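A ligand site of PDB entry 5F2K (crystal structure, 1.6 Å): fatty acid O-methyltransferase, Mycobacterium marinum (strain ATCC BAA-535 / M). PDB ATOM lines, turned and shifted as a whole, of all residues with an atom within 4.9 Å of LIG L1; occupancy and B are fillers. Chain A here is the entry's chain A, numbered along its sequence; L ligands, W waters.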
ATOM      1  N   PRO A  18      -2.878 -13.659 -23.077  1.00  0.00           N
ATOM      2  CA  PRO A  18      -2.863 -13.562 -21.610  1.00  0.00           C
ATOM      3  C   PRO A  18      -3.722 -12.409 -21.110  1.00  0.00           C
ATOM      4  O   PRO A  18      -4.254 -11.634 -21.905  1.00  0.00           O
ATOM      5  CB  PRO A  18      -1.389 -13.293 -21.269  1.00  0.00           C
ATOM      6  CG  PRO A  18      -0.622 -13.511 -22.519  1.00  0.00           C
ATOM      7  CD  PRO A  18      -1.562 -13.357 -23.672  1.00  0.00           C
ATOM      8  N   MET A  19      -3.856 -12.303 -19.779  1.00  0.00           N
ATOM      9  CA  MET A  19      -4.668 -11.239 -19.180  1.00  0.00           C
ATOM     10  C   MET A  19      -3.995  -9.885 -19.398  1.00  0.00           C
ATOM     11  O   MET A  19      -2.787  -9.817 -19.618  1.00  0.00           O
ATOM     12  CB  MET A  19      -4.869 -11.510 -17.686  1.00  0.00           C
ATOM     13  CG  MET A  19      -5.270 -12.941 -17.323  1.00  0.00           C
ATOM     14  SD  MET A  19      -6.899 -13.443 -17.923  1.00  0.00           S
ATOM     15  CE  MET A  19      -6.552 -14.141 -19.531  1.00  0.00           C
ATOM     16  N   TYR A  24      -5.434  -6.475 -14.586  1.00  0.00           N
ATOM     17  CA  TYR A  24      -5.908  -7.724 -13.986  1.00  0.00           C
ATOM     18  C   TYR A  24      -5.948  -7.736 -12.449  1.00  0.00           C
ATOM     19  O   TYR A  24      -6.914  -8.219 -11.864  1.00  0.00           O
ATOM     20  CB  TYR A  24      -5.156  -8.965 -14.528  1.00  0.00           C
ATOM     21  CG  TYR A  24      -5.846 -10.253 -14.137  1.00  0.00           C
ATOM     22  CD1 TYR A  24      -6.958 -10.721 -14.851  1.00  0.00           C
ATOM     23  CD2 TYR A  24      -5.422 -10.998 -13.027  1.00  0.00           C
ATOM     24  CE1 TYR A  24      -7.613 -11.888 -14.494  1.00  0.00           C
ATOM     25  CE2 TYR A  24      -6.067 -12.164 -12.660  1.00  0.00           C
ATOM     26  CZ  TYR A  24      -7.163 -12.609 -13.393  1.00  0.00           C
ATOM     27  OH  TYR A  24      -7.819 -13.767 -13.026  1.00  0.00           O
ATOM     28  N   SER A  28      -9.971  -8.416 -10.872  1.00  0.00           N
ATOM     29  CA  SER A  28     -10.158  -9.858 -10.683  1.00  0.00           C
ATOM     30  C   SER A  28     -10.786 -10.228  -9.335  1.00  0.00           C
ATOM     31  O   SER A  28     -10.561 -11.323  -8.796  1.00  0.00           O
ATOM     32  CB  SER A  28      -8.834 -10.605 -10.903  1.00  0.00           C
ATOM     33  OG  SER A  28      -7.822 -10.115 -10.048  1.00  0.00           O
ATOM     34  N   GLN A  31     -13.145 -13.243  -9.726  1.00  0.00           N
ATOM     35  CA  GLN A  31     -12.363 -14.476  -9.658  1.00  0.00           C
ATOM     36  C   GLN A  31     -11.961 -14.821  -8.236  1.00  0.00           C
ATOM     37  O   GLN A  31     -12.101 -15.963  -7.793  1.00  0.00           O
ATOM     38  CB  GLN A  31     -11.125 -14.397 -10.567  1.00  0.00           C
ATOM     39  CG  GLN A  31     -11.423 -14.344 -12.062  1.00  0.00           C
ATOM     40  CD  GLN A  31     -11.505 -12.919 -12.603  1.00  0.00           C
ATOM     41  OE1 GLN A  31     -12.065 -12.025 -11.973  1.00  0.00           O
ATOM     42  NE2 GLN A  31     -10.957 -12.716 -13.798  1.00  0.00           N
ATOM     43  N   LEU A  35     -13.185 -18.287  -6.175  1.00  0.00           N
ATOM     44  CA  LEU A  35     -12.217 -19.340  -5.841  1.00  0.00           C
ATOM     45  C   LEU A  35     -12.137 -19.597  -4.331  1.00  0.00           C
ATOM     46  O   LEU A  35     -11.520 -20.576  -3.890  1.00  0.00           O
ATOM     47  CB  LEU A  35     -10.825 -19.029  -6.432  1.00  0.00           C
ATOM     48  CG  LEU A  35     -10.032 -17.794  -5.986  1.00  0.00           C
ATOM     49  CD1 LEU A  35      -9.297 -18.057  -4.669  1.00  0.00           C
ATOM     50  CD2 LEU A  35      -9.036 -17.391  -7.061  1.00  0.00           C
ATOM     51  N   ASP A  62       1.428 -23.461  -8.979  1.00  0.00           N
ATOM     52  CA  ASP A  62       0.285 -22.587  -9.246  1.00  0.00           C
ATOM     53  C   ASP A  62       0.146 -22.471 -10.756  1.00  0.00           C
ATOM     54  O   ASP A  62       0.874 -21.716 -11.393  1.00  0.00           O
ATOM     55  CB  ASP A  62       0.509 -21.214  -8.575  1.00  0.00           C
ATOM     56  CG  ASP A  62      -0.500 -20.148  -8.990  1.00  0.00           C
ATOM     57  OD1 ASP A  62      -1.655 -20.471  -9.342  1.00  0.00           O
ATOM     58  OD2 ASP A  62      -0.138 -18.949  -8.915  1.00  0.00           O
ATOM     59  N   GLY A  64      -1.293 -21.270 -13.989  1.00  0.00           N
ATOM     60  CA  GLY A  64      -2.062 -20.153 -14.554  1.00  0.00           C
ATOM     61  C   GLY A  64      -2.094 -18.957 -13.630  1.00  0.00           C
ATOM     62  O   GLY A  64      -3.162 -18.502 -13.223  1.00  0.00           O
ATOM     63  N   VAL A  65      -0.912 -18.417 -13.338  1.00  0.00           N
ATOM     64  CA  VAL A  65      -0.740 -17.371 -12.319  1.00  0.00           C
ATOM     65  C   VAL A  65      -1.209 -15.946 -12.707  1.00  0.00           C
ATOM     66  O   VAL A  65      -1.589 -15.169 -11.837  1.00  0.00           O
ATOM     67  CB  VAL A  65       0.733 -17.326 -11.824  1.00  0.00           C
ATOM     68  CG1 VAL A  65       1.706 -16.995 -12.962  1.00  0.00           C
ATOM     69  CG2 VAL A  65       0.901 -16.354 -10.662  1.00  0.00           C
ATOM     70  N   ALA A  66      -1.162 -15.616 -13.994  1.00  0.00           N
ATOM     71  CA  ALA A  66      -1.328 -14.222 -14.450  1.00  0.00           C
ATOM     72  C   ALA A  66      -0.391 -13.295 -13.661  1.00  0.00           C
ATOM     73  O   ALA A  66       0.808 -13.557 -13.592  1.00  0.00           O
ATOM     74  CB  ALA A  66      -2.796 -13.785 -14.357  1.00  0.00           C
ATOM     75  N   ASN A  70      -4.281 -13.070  -7.324  1.00  0.00           N
ATOM     76  CA  ASN A  70      -5.207 -14.039  -6.739  1.00  0.00           C
ATOM     77  C   ASN A  70      -4.555 -15.330  -6.273  1.00  0.00           C
ATOM     78  O   ASN A  70      -5.241 -16.262  -5.864  1.00  0.00           O
ATOM     79  CB  ASN A  70      -6.341 -14.364  -7.711  1.00  0.00           C
ATOM     80  CG  ASN A  70      -7.388 -13.267  -7.780  1.00  0.00           C
ATOM     81  OD1 ASN A  70      -7.419 -12.372  -6.918  1.00  0.00           O
ATOM     82  ND2 ASN A  70      -8.237 -13.321  -8.791  1.00  0.00           N
ATOM     83  N   SER A  71      -3.225 -15.366  -6.306  1.00  0.00           N
ATOM     84  CA  SER A  71      -2.497 -16.540  -5.842  1.00  0.00           C
ATOM     85  C   SER A  71      -2.073 -16.409  -4.378  1.00  0.00           C
ATOM     86  O   SER A  71      -1.817 -17.410  -3.716  1.00  0.00           O
ATOM     87  CB  SER A  71      -1.294 -16.799  -6.734  1.00  0.00           C
ATOM     88  OG  SER A  71      -1.707 -17.079  -8.057  1.00  0.00           O
ATOM     89  N   THR A  97       3.127 -20.819 -12.752  1.00  0.00           N
ATOM     90  CA  THR A  97       3.250 -21.123 -14.179  1.00  0.00           C
ATOM     91  C   THR A  97       2.246 -20.363 -15.033  1.00  0.00           C
ATOM     92  O   THR A  97       1.131 -20.081 -14.603  1.00  0.00           O
ATOM     93  CB  THR A  97       3.206 -22.647 -14.476  1.00  0.00           C
ATOM     94  OG1 THR A  97       1.865 -23.081 -14.751  1.00  0.00           O
ATOM     95  CG2 THR A  97       3.771 -23.461 -13.323  1.00  0.00           C
ATOM     96  N   ASP A  98       2.669 -20.007 -16.250  1.00  0.00           N
ATOM     97  CA  ASP A  98       1.774 -19.390 -17.225  1.00  0.00           C
ATOM     98  C   ASP A  98       2.358 -19.611 -18.614  1.00  0.00           C
ATOM     99  O   ASP A  98       3.274 -20.412 -18.792  1.00  0.00           O
ATOM    100  CB  ASP A  98       1.576 -17.897 -16.908  1.00  0.00           C
ATOM    101  CG  ASP A  98       0.181 -17.408 -17.258  1.00  0.00           C
ATOM    102  OD1 ASP A  98      -0.060 -17.123 -18.450  1.00  0.00           O
ATOM    103  OD2 ASP A  98      -0.665 -17.295 -16.349  1.00  0.00           O
ATOM    104  N   VAL A  99       1.811 -18.911 -19.600  1.00  0.00           N
ATOM    105  CA  VAL A  99       2.356 -18.946 -20.961  1.00  0.00           C
ATOM    106  C   VAL A  99       3.562 -17.986 -21.064  1.00  0.00           C
ATOM    107  O   VAL A  99       3.699 -17.078 -20.236  1.00  0.00           O
ATOM    108  CB  VAL A  99       1.271 -18.615 -22.014  1.00  0.00           C
ATOM    109  CG1 VAL A  99       0.174 -19.665 -21.972  1.00  0.00           C
ATOM    110  CG2 VAL A  99       0.688 -17.234 -21.794  1.00  0.00           C
ATOM    111  N   ASN A 102       2.917 -14.165 -20.815  1.00  0.00           N
ATOM    112  CA  ASN A 102       2.404 -13.572 -19.582  1.00  0.00           C
ATOM    113  C   ASN A 102       3.393 -12.512 -19.090  1.00  0.00           C
ATOM    114  O   ASN A 102       4.597 -12.607 -19.349  1.00  0.00           O
ATOM    115  CB  ASN A 102       2.212 -14.648 -18.501  1.00  0.00           C
ATOM    116  CG  ASN A 102       1.676 -14.086 -17.192  1.00  0.00           C
ATOM    117  OD1 ASN A 102       0.672 -13.374 -17.173  1.00  0.00           O
ATOM    118  ND2 ASN A 102       2.354 -14.410 -16.086  1.00  0.00           N
ATOM    119  N   ARG A 132       5.834 -21.752 -19.736  1.00  0.00           N
ATOM    120  CA  ARG A 132       5.675 -22.840 -20.711  1.00  0.00           C
ATOM    121  C   ARG A 132       4.263 -23.383 -20.536  1.00  0.00           C
ATOM    122  O   ARG A 132       3.845 -23.637 -19.409  1.00  0.00           O
ATOM    123  CB  ARG A 132       6.674 -23.959 -20.426  1.00  0.00           C
ATOM    124  CG  ARG A 132       8.135 -23.535 -20.382  1.00  0.00           C
ATOM    125  CD  ARG A 132       9.020 -24.688 -19.952  1.00  0.00           C
ATOM    126  NE  ARG A 132       9.126 -25.701 -20.996  1.00  0.00           N
ATOM    127  CZ  ARG A 132       9.487 -26.956 -20.788  1.00  0.00           C
ATOM    128  NH1 ARG A 132       9.775 -27.391 -19.568  1.00  0.00           N
ATOM    129  NH2 ARG A 132       9.550 -27.800 -21.817  1.00  0.00           N
ATOM    130  N   SER A 133       3.523 -23.541 -21.635  1.00  0.00           N
ATOM    131  CA  SER A 133       2.144 -24.029 -21.580  1.00  0.00           C
ATOM    132  C   SER A 133       1.975 -25.234 -20.658  1.00  0.00           C
ATOM    133  O   SER A 133       2.726 -26.212 -20.757  1.00  0.00           O
ATOM    134  CB  SER A 133       1.649 -24.400 -22.977  1.00  0.00           C
ATOM    135  OG  SER A 133       0.365 -25.021 -22.893  1.00  0.00           O
ATOM    136  N   PHE A 134       0.974 -25.180 -19.778  1.00  0.00           N
ATOM    137  CA  PHE A 134       0.710 -26.299 -18.868  1.00  0.00           C
ATOM    138  C   PHE A 134       0.021 -27.506 -19.545  1.00  0.00           C
ATOM    139  O   PHE A 134      -0.332 -28.478 -18.877  1.00  0.00           O
ATOM    140  CB  PHE A 134       0.031 -25.874 -17.548  1.00  0.00           C
ATOM    141  CG  PHE A 134      -1.276 -25.127 -17.707  1.00  0.00           C
ATOM    142  CD1 PHE A 134      -2.253 -25.534 -18.629  1.00  0.00           C
ATOM    143  CD2 PHE A 134      -1.559 -24.048 -16.879  1.00  0.00           C
ATOM    144  CE1 PHE A 134      -3.454 -24.844 -18.742  1.00  0.00           C
ATOM    145  CE2 PHE A 134      -2.757 -23.354 -16.976  1.00  0.00           C
ATOM    146  CZ  PHE A 134      -3.701 -23.753 -17.911  1.00  0.00           C
ATOM    147  N   TYR A 135      -0.142 -27.443 -20.865  1.00  0.00           N
ATOM    148  CA  TYR A 135      -0.596 -28.617 -21.614  1.00  0.00           C
ATOM    149  C   TYR A 135       0.547 -29.546 -22.018  1.00  0.00           C
ATOM    150  O   TYR A 135       0.365 -30.467 -22.800  1.00  0.00           O
ATOM    151  CB  TYR A 135      -1.468 -28.203 -22.815  1.00  0.00           C
ATOM    152  CG  TYR A 135      -2.755 -27.542 -22.369  1.00  0.00           C
ATOM    153  CD1 TYR A 135      -3.651 -28.212 -21.535  1.00  0.00           C
ATOM    154  CD2 TYR A 135      -3.066 -26.238 -22.770  1.00  0.00           C
ATOM    155  CE1 TYR A 135      -4.823 -27.611 -21.111  1.00  0.00           C
ATOM    156  CE2 TYR A 135      -4.242 -25.631 -22.353  1.00  0.00           C
ATOM    157  CZ  TYR A 135      -5.121 -26.325 -21.522  1.00  0.00           C
ATOM    158  OH  TYR A 135      -6.293 -25.724 -21.098  1.00  0.00           O
ATOM    159  N   SER A 150      -6.575 -22.078 -10.590  1.00  0.00           N
ATOM    160  CA  SER A 150      -7.867 -21.401 -10.585  1.00  0.00           C
ATOM    161  C   SER A 150      -8.076 -20.545 -11.819  1.00  0.00           C
ATOM    162  O   SER A 150      -7.186 -19.776 -12.220  1.00  0.00           O
ATOM    163  CB  SER A 150      -8.056 -20.592  -9.301  1.00  0.00           C
ATOM    164  OG  SER A 150      -7.012 -19.643  -9.120  1.00  0.00           O
ATOM    165  N   TRP A 151      -9.251 -20.675 -12.428  1.00  0.00           N
ATOM    166  CA  TRP A 151      -9.681 -19.843 -13.546  1.00  0.00           C
ATOM    167  C   TRP A 151      -8.765 -19.915 -14.774  1.00  0.00           C
ATOM    168  O   TRP A 151      -8.688 -18.954 -15.560  1.00  0.00           O
ATOM    169  CB  TRP A 151      -9.821 -18.387 -13.091  1.00  0.00           C
ATOM    170  CG  TRP A 151     -10.949 -18.120 -12.135  1.00  0.00           C
ATOM    171  CD1 TRP A 151     -10.873 -18.061 -10.770  1.00  0.00           C
ATOM    172  CD2 TRP A 151     -12.306 -17.830 -12.480  1.00  0.00           C
ATOM    173  NE1 TRP A 151     -12.115 -17.758 -10.243  1.00  0.00           N
ATOM    174  CE2 TRP A 151     -13.004 -17.615 -11.276  1.00  0.00           C
ATOM    175  CE3 TRP A 151     -12.999 -17.736 -13.692  1.00  0.00           C
ATOM    176  CZ2 TRP A 151     -14.370 -17.305 -11.240  1.00  0.00           C
ATOM    177  CZ3 TRP A 151     -14.351 -17.430 -13.670  1.00  0.00           C
ATOM    178  CH2 TRP A 151     -15.030 -17.211 -12.446  1.00  0.00           C
ATOM    179  N   ALA A 152      -8.087 -21.045 -14.947  1.00  0.00           N
ATOM    180  CA  ALA A 152      -7.101 -21.196 -16.023  1.00  0.00           C
ATOM    181  C   ALA A 152      -7.418 -22.263 -17.058  1.00  0.00           C
ATOM    182  O   ALA A 152      -7.216 -22.044 -18.259  1.00  0.00           O
ATOM    183  CB  ALA A 152      -5.705 -21.437 -15.438  1.00  0.00           C
ATOM    184  N   TRP A 155      -9.340 -22.142 -20.555  1.00  0.00           N
ATOM    185  CA  TRP A 155      -8.670 -21.626 -21.739  1.00  0.00           C
ATOM    186  C   TRP A 155      -8.129 -22.758 -22.599  1.00  0.00           C
ATOM    187  O   TRP A 155      -7.239 -23.519 -22.177  1.00  0.00           O
ATOM    188  CB  TRP A 155      -7.538 -20.671 -21.357  1.00  0.00           C
ATOM    189  CG  TRP A 155      -8.032 -19.375 -20.794  1.00  0.00           C
ATOM    190  CD1 TRP A 155      -8.160 -19.046 -19.474  1.00  0.00           C
ATOM    191  CD2 TRP A 155      -8.500 -18.236 -21.541  1.00  0.00           C
ATOM    192  NE1 TRP A 155      -8.678 -17.770 -19.359  1.00  0.00           N
ATOM    193  CE2 TRP A 155      -8.893 -17.259 -20.601  1.00  0.00           C
ATOM    194  CE3 TRP A 155      -8.620 -17.958 -22.917  1.00  0.00           C
ATOM    195  CZ2 TRP A 155      -9.392 -16.008 -20.992  1.00  0.00           C
ATOM    196  CZ3 TRP A 155      -9.114 -16.712 -23.301  1.00  0.00           C
ATOM    197  CH2 TRP A 155      -9.489 -15.746 -22.338  1.00  0.00           C
HETATM  198  N1  LIG L   1      -5.140 -18.005 -11.206  1.00  0.00           N
HETATM  199  C1  LIG L   1      -5.472 -16.577 -11.351  1.00  0.00           C
HETATM  200  C2  LIG L   1      -5.347 -16.145 -12.817  1.00  0.00           C
HETATM  201  C3  LIG L   1      -6.407 -16.751 -13.746  1.00  0.00           C
HETATM  202  S1  LIG L   1      -6.412 -15.899 -15.304  1.00  0.00           S
HETATM  203  C4  LIG L   1      -6.826 -16.270 -10.765  1.00  0.00           C
HETATM  204  O1  LIG L   1      -7.492 -17.134 -10.189  1.00  0.00           O
HETATM  205  O2  LIG L   1      -7.302 -15.134 -10.845  1.00  0.00           O
HETATM  206  C5  LIG L   1      -6.135 -17.209 -16.453  1.00  0.00           C
HETATM  207  C6  LIG L   1      -4.639 -17.467 -16.670  1.00  0.00           C
HETATM  208  O3  LIG L   1      -4.459 -18.752 -17.278  1.00  0.00           O
HETATM  209  C7  LIG L   1      -4.003 -16.438 -17.597  1.00  0.00           C
HETATM  210  O4  LIG L   1      -2.841 -15.845 -17.009  1.00  0.00           O
HETATM  211  C8  LIG L   1      -3.612 -17.245 -18.827  1.00  0.00           C
HETATM  212  O5  LIG L   1      -2.479 -16.740 -19.526  1.00  0.00           O
HETATM  213  C9  LIG L   1      -3.376 -18.611 -18.197  1.00  0.00           C
HETATM  214  N2  LIG L   1      -3.330 -19.671 -19.215  1.00  0.00           N
HETATM  215  C10 LIG L   1      -4.208 -19.907 -20.210  1.00  0.00           C
HETATM  216  N3  LIG L   1      -3.806 -20.963 -20.958  1.00  0.00           N
HETATM  217  C11 LIG L   1      -2.645 -21.397 -20.443  1.00  0.00           C
HETATM  218  C12 LIG L   1      -1.673 -22.473 -20.739  1.00  0.00           C
HETATM  219  N4  LIG L   1      -1.876 -23.299 -21.792  1.00  0.00           N
HETATM  220  N5  LIG L   1      -0.585 -22.589 -19.939  1.00  0.00           N
HETATM  221  C13 LIG L   1      -0.362 -21.760 -18.895  1.00  0.00           C
HETATM  222  N6  LIG L   1      -1.207 -20.761 -18.571  1.00  0.00           N
HETATM  223  C14 LIG L   1      -2.332 -20.549 -19.291  1.00  0.00           C
HETATM  224  C1  LG2 L   2     -10.276 -15.527 -16.228  1.00  0.00           C
HETATM  225  C2  LG2 L   2     -11.777 -15.258 -16.205  1.00  0.00           C
HETATM  226  C3  LG2 L   2     -12.470 -15.539 -17.546  1.00  0.00           C
HETATM  227  C4  LG2 L   2     -13.923 -15.107 -17.496  1.00  0.00           C
HETATM  228  C5  LG2 L   2     -14.643 -15.365 -18.814  1.00  0.00           C
HETATM  229  C6  LG2 L   2     -16.056 -14.782 -18.788  1.00  0.00           C
HETATM  230  C7  LG2 L   2     -16.804 -15.078 -20.093  1.00  0.00           C
HETATM  231  C8  LG2 L   2     -18.121 -14.342 -20.152  1.00  0.00           C
HETATM  232  O1  LG2 L   2      -9.776 -16.271 -17.100  1.00  0.00           O
HETATM  233  O2  LG2 L   2      -9.576 -14.985 -15.338  1.00  0.00           O
HETATM  234  O   HOH W   1      -3.955 -20.745 -10.930  1.00  0.00           O
HETATM  235  O   HOH W   2      -2.974 -17.364 -22.213  1.00  0.00           O
HETATM  236  O   HOH W   3      -4.073 -22.015 -23.519  1.00  0.00           O
HETATM  237  O   HOH W   4      -3.041 -14.984  -9.465  1.00  0.00           O
HETATM  238  O   HOH W   5      -4.090 -18.472  -8.612  1.00  0.00           O
HETATM  239  O   HOH W   6      -1.992 -13.416 -17.928  1.00  0.00           O
HETATM  240  O   HOH W   7       2.191 -22.852 -17.500  1.00  0.00           O
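The side-chain carboxylate of Asp 98 sits at hydrogen-bond distance from an oxygen (O5) of LIG L1, 2.7 Å away. N of Ala 66 sits close to O4 of LIG L1, at 3.5 Å. OH of Tyr 24 lies within hydrogen-bond range of O2 of LG2 L2 (3.1 Å). N of Phe 134 is in hydrogen-bond range of N5 of LIG L1, at 3.0 Å. N1 of LIG L1 sits at hydrogen-bond distance from O of Ser 150. NE1 of Trp 155 lies within hydrogen-bond range of O1 of LG2 L2. The side-chain hydroxyl of Tyr 24 is in hydrogen-bond range of an oxygen (O2) of LIG L1 (2.6 Å). O2 of LG2 L2 lies within hydrogen-bond range of NE2 of Gln 31 (3.1 Å). A nitrogen (N4) of LIG L1 lies within hydrogen-bond range of the side-chain hydroxyl of Ser 133. An oxygen (O1) of LIG L1 lies within hydrogen-bond range of the side-chain hydroxyl (OG) of Ser 150. O of Gly 64 is in hydrogen-bond range of N1 of LIG L1, at 2.9 Å. ND2 of Asn 70 is in hydrogen-bond range of O2 of LIG L1, at 2.9 Å.
The backbone NH (N) of Ala 66 is in hydrogen-bond range of the side-chain carboxylate (OD2) of Asp 98 (2.9 Å). The indole nitrogen of Trp 151 lies within hydrogen-bond range of the backbone carbonyl oxygen of Gln 31. OH of Tyr 135 is in hydrogen-bond range of O of Trp 155 (2.6 Å). The backbone carbonyl oxygen of Tyr 24 is in hydrogen-bond range of the side-chain hydroxyl of Ser 28, 2.8 Å away. OG of Ser 133 lies close to N of Tyr 135. O of Asp 98 is in hydrogen-bond range of N of Arg 132. N of Val 65 lies within hydrogen-bond range of OD2 of Asp 98. The side-chain amide nitrogen (ND2) of Asn 102 lies within hydrogen-bond range of the backbone carbonyl oxygen (O) of Ala 66 (3.1 Å).
SD of Met 19 lies close to S1 of LIG L1, at 3.6 Å. CA of Pro 18 touches O5 of LIG L1 (3.8 Å). Gln 31 touches LIG L1 (CB to O2, 3.9 Å). CD2 of Leu 35 touches O1 of LIG L1, at 3.5 Å. CG1 of Val 99 touches C12 of LIG L1, 3.6 Å away. Tyr 135 touches LIG L1. Trp 151 touches LIG L1 (O to C5, 3.2 Å). Ala 152 touches LIG L1 (CB to O3, 3.5 Å). Trp 155 touches LIG L1. Hydrophobic or aromatic side chains that line LIG L1: Met 19, Tyr 24, Leu 35, Ala 66, Val 99, Phe 134, Tyr 135, Trp 151, Ala 152 and Trp 155. 17 residues have an atom within 4 Å of LIG L1: Pro 18, Met 19, Tyr 24, Gln 31, Leu 35, Gly 64, Ala 66, Asn 70, Asp 98, Val 99, Ser 133, Phe 134, Tyr 135, Ser 150, Trp 151, Ala 152 and Trp 155. The nearest printed residue that does not touch LIG L1 is Val 65 (4.004 Å).
Water W6 lies within hydrogen-bond range of an oxygen (O4) of LIG L1, the side-chain amide oxygen (OD1) of Asn 102 and the backbone NH (N) of Met 19. Water W5 lies within hydrogen-bond range of the side-chain hydroxyl (OG) of Ser 71 (2.8 Å), a nitrogen (N1) of LIG L1 (2.8 Å), the side-chain hydroxyl (OG) of Ser 150 (3.2 Å) and the side-chain carboxylate (OD1) of Asp 62 (3.2 Å). Water W1 lies within hydrogen-bond range of OD1 of Asp 62, N of Ser 150, N1 of LIG L1 and O of Gly 64. Water W7 lies within hydrogen-bond range of the backbone carbonyl oxygen of Arg 132 (2.6 Å), the side-chain hydroxyl of Thr 97 (2.8 Å), the backbone carbonyl oxygen of Asp 98 (3.0 Å) and the backbone NH of Phe 134 (3.5 Å). Water W4 lies within hydrogen-bond range of O of Val 65 (2.8 Å), OG of Ser 71 (2.9 Å) and N of Asn 70 (3.1 Å).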
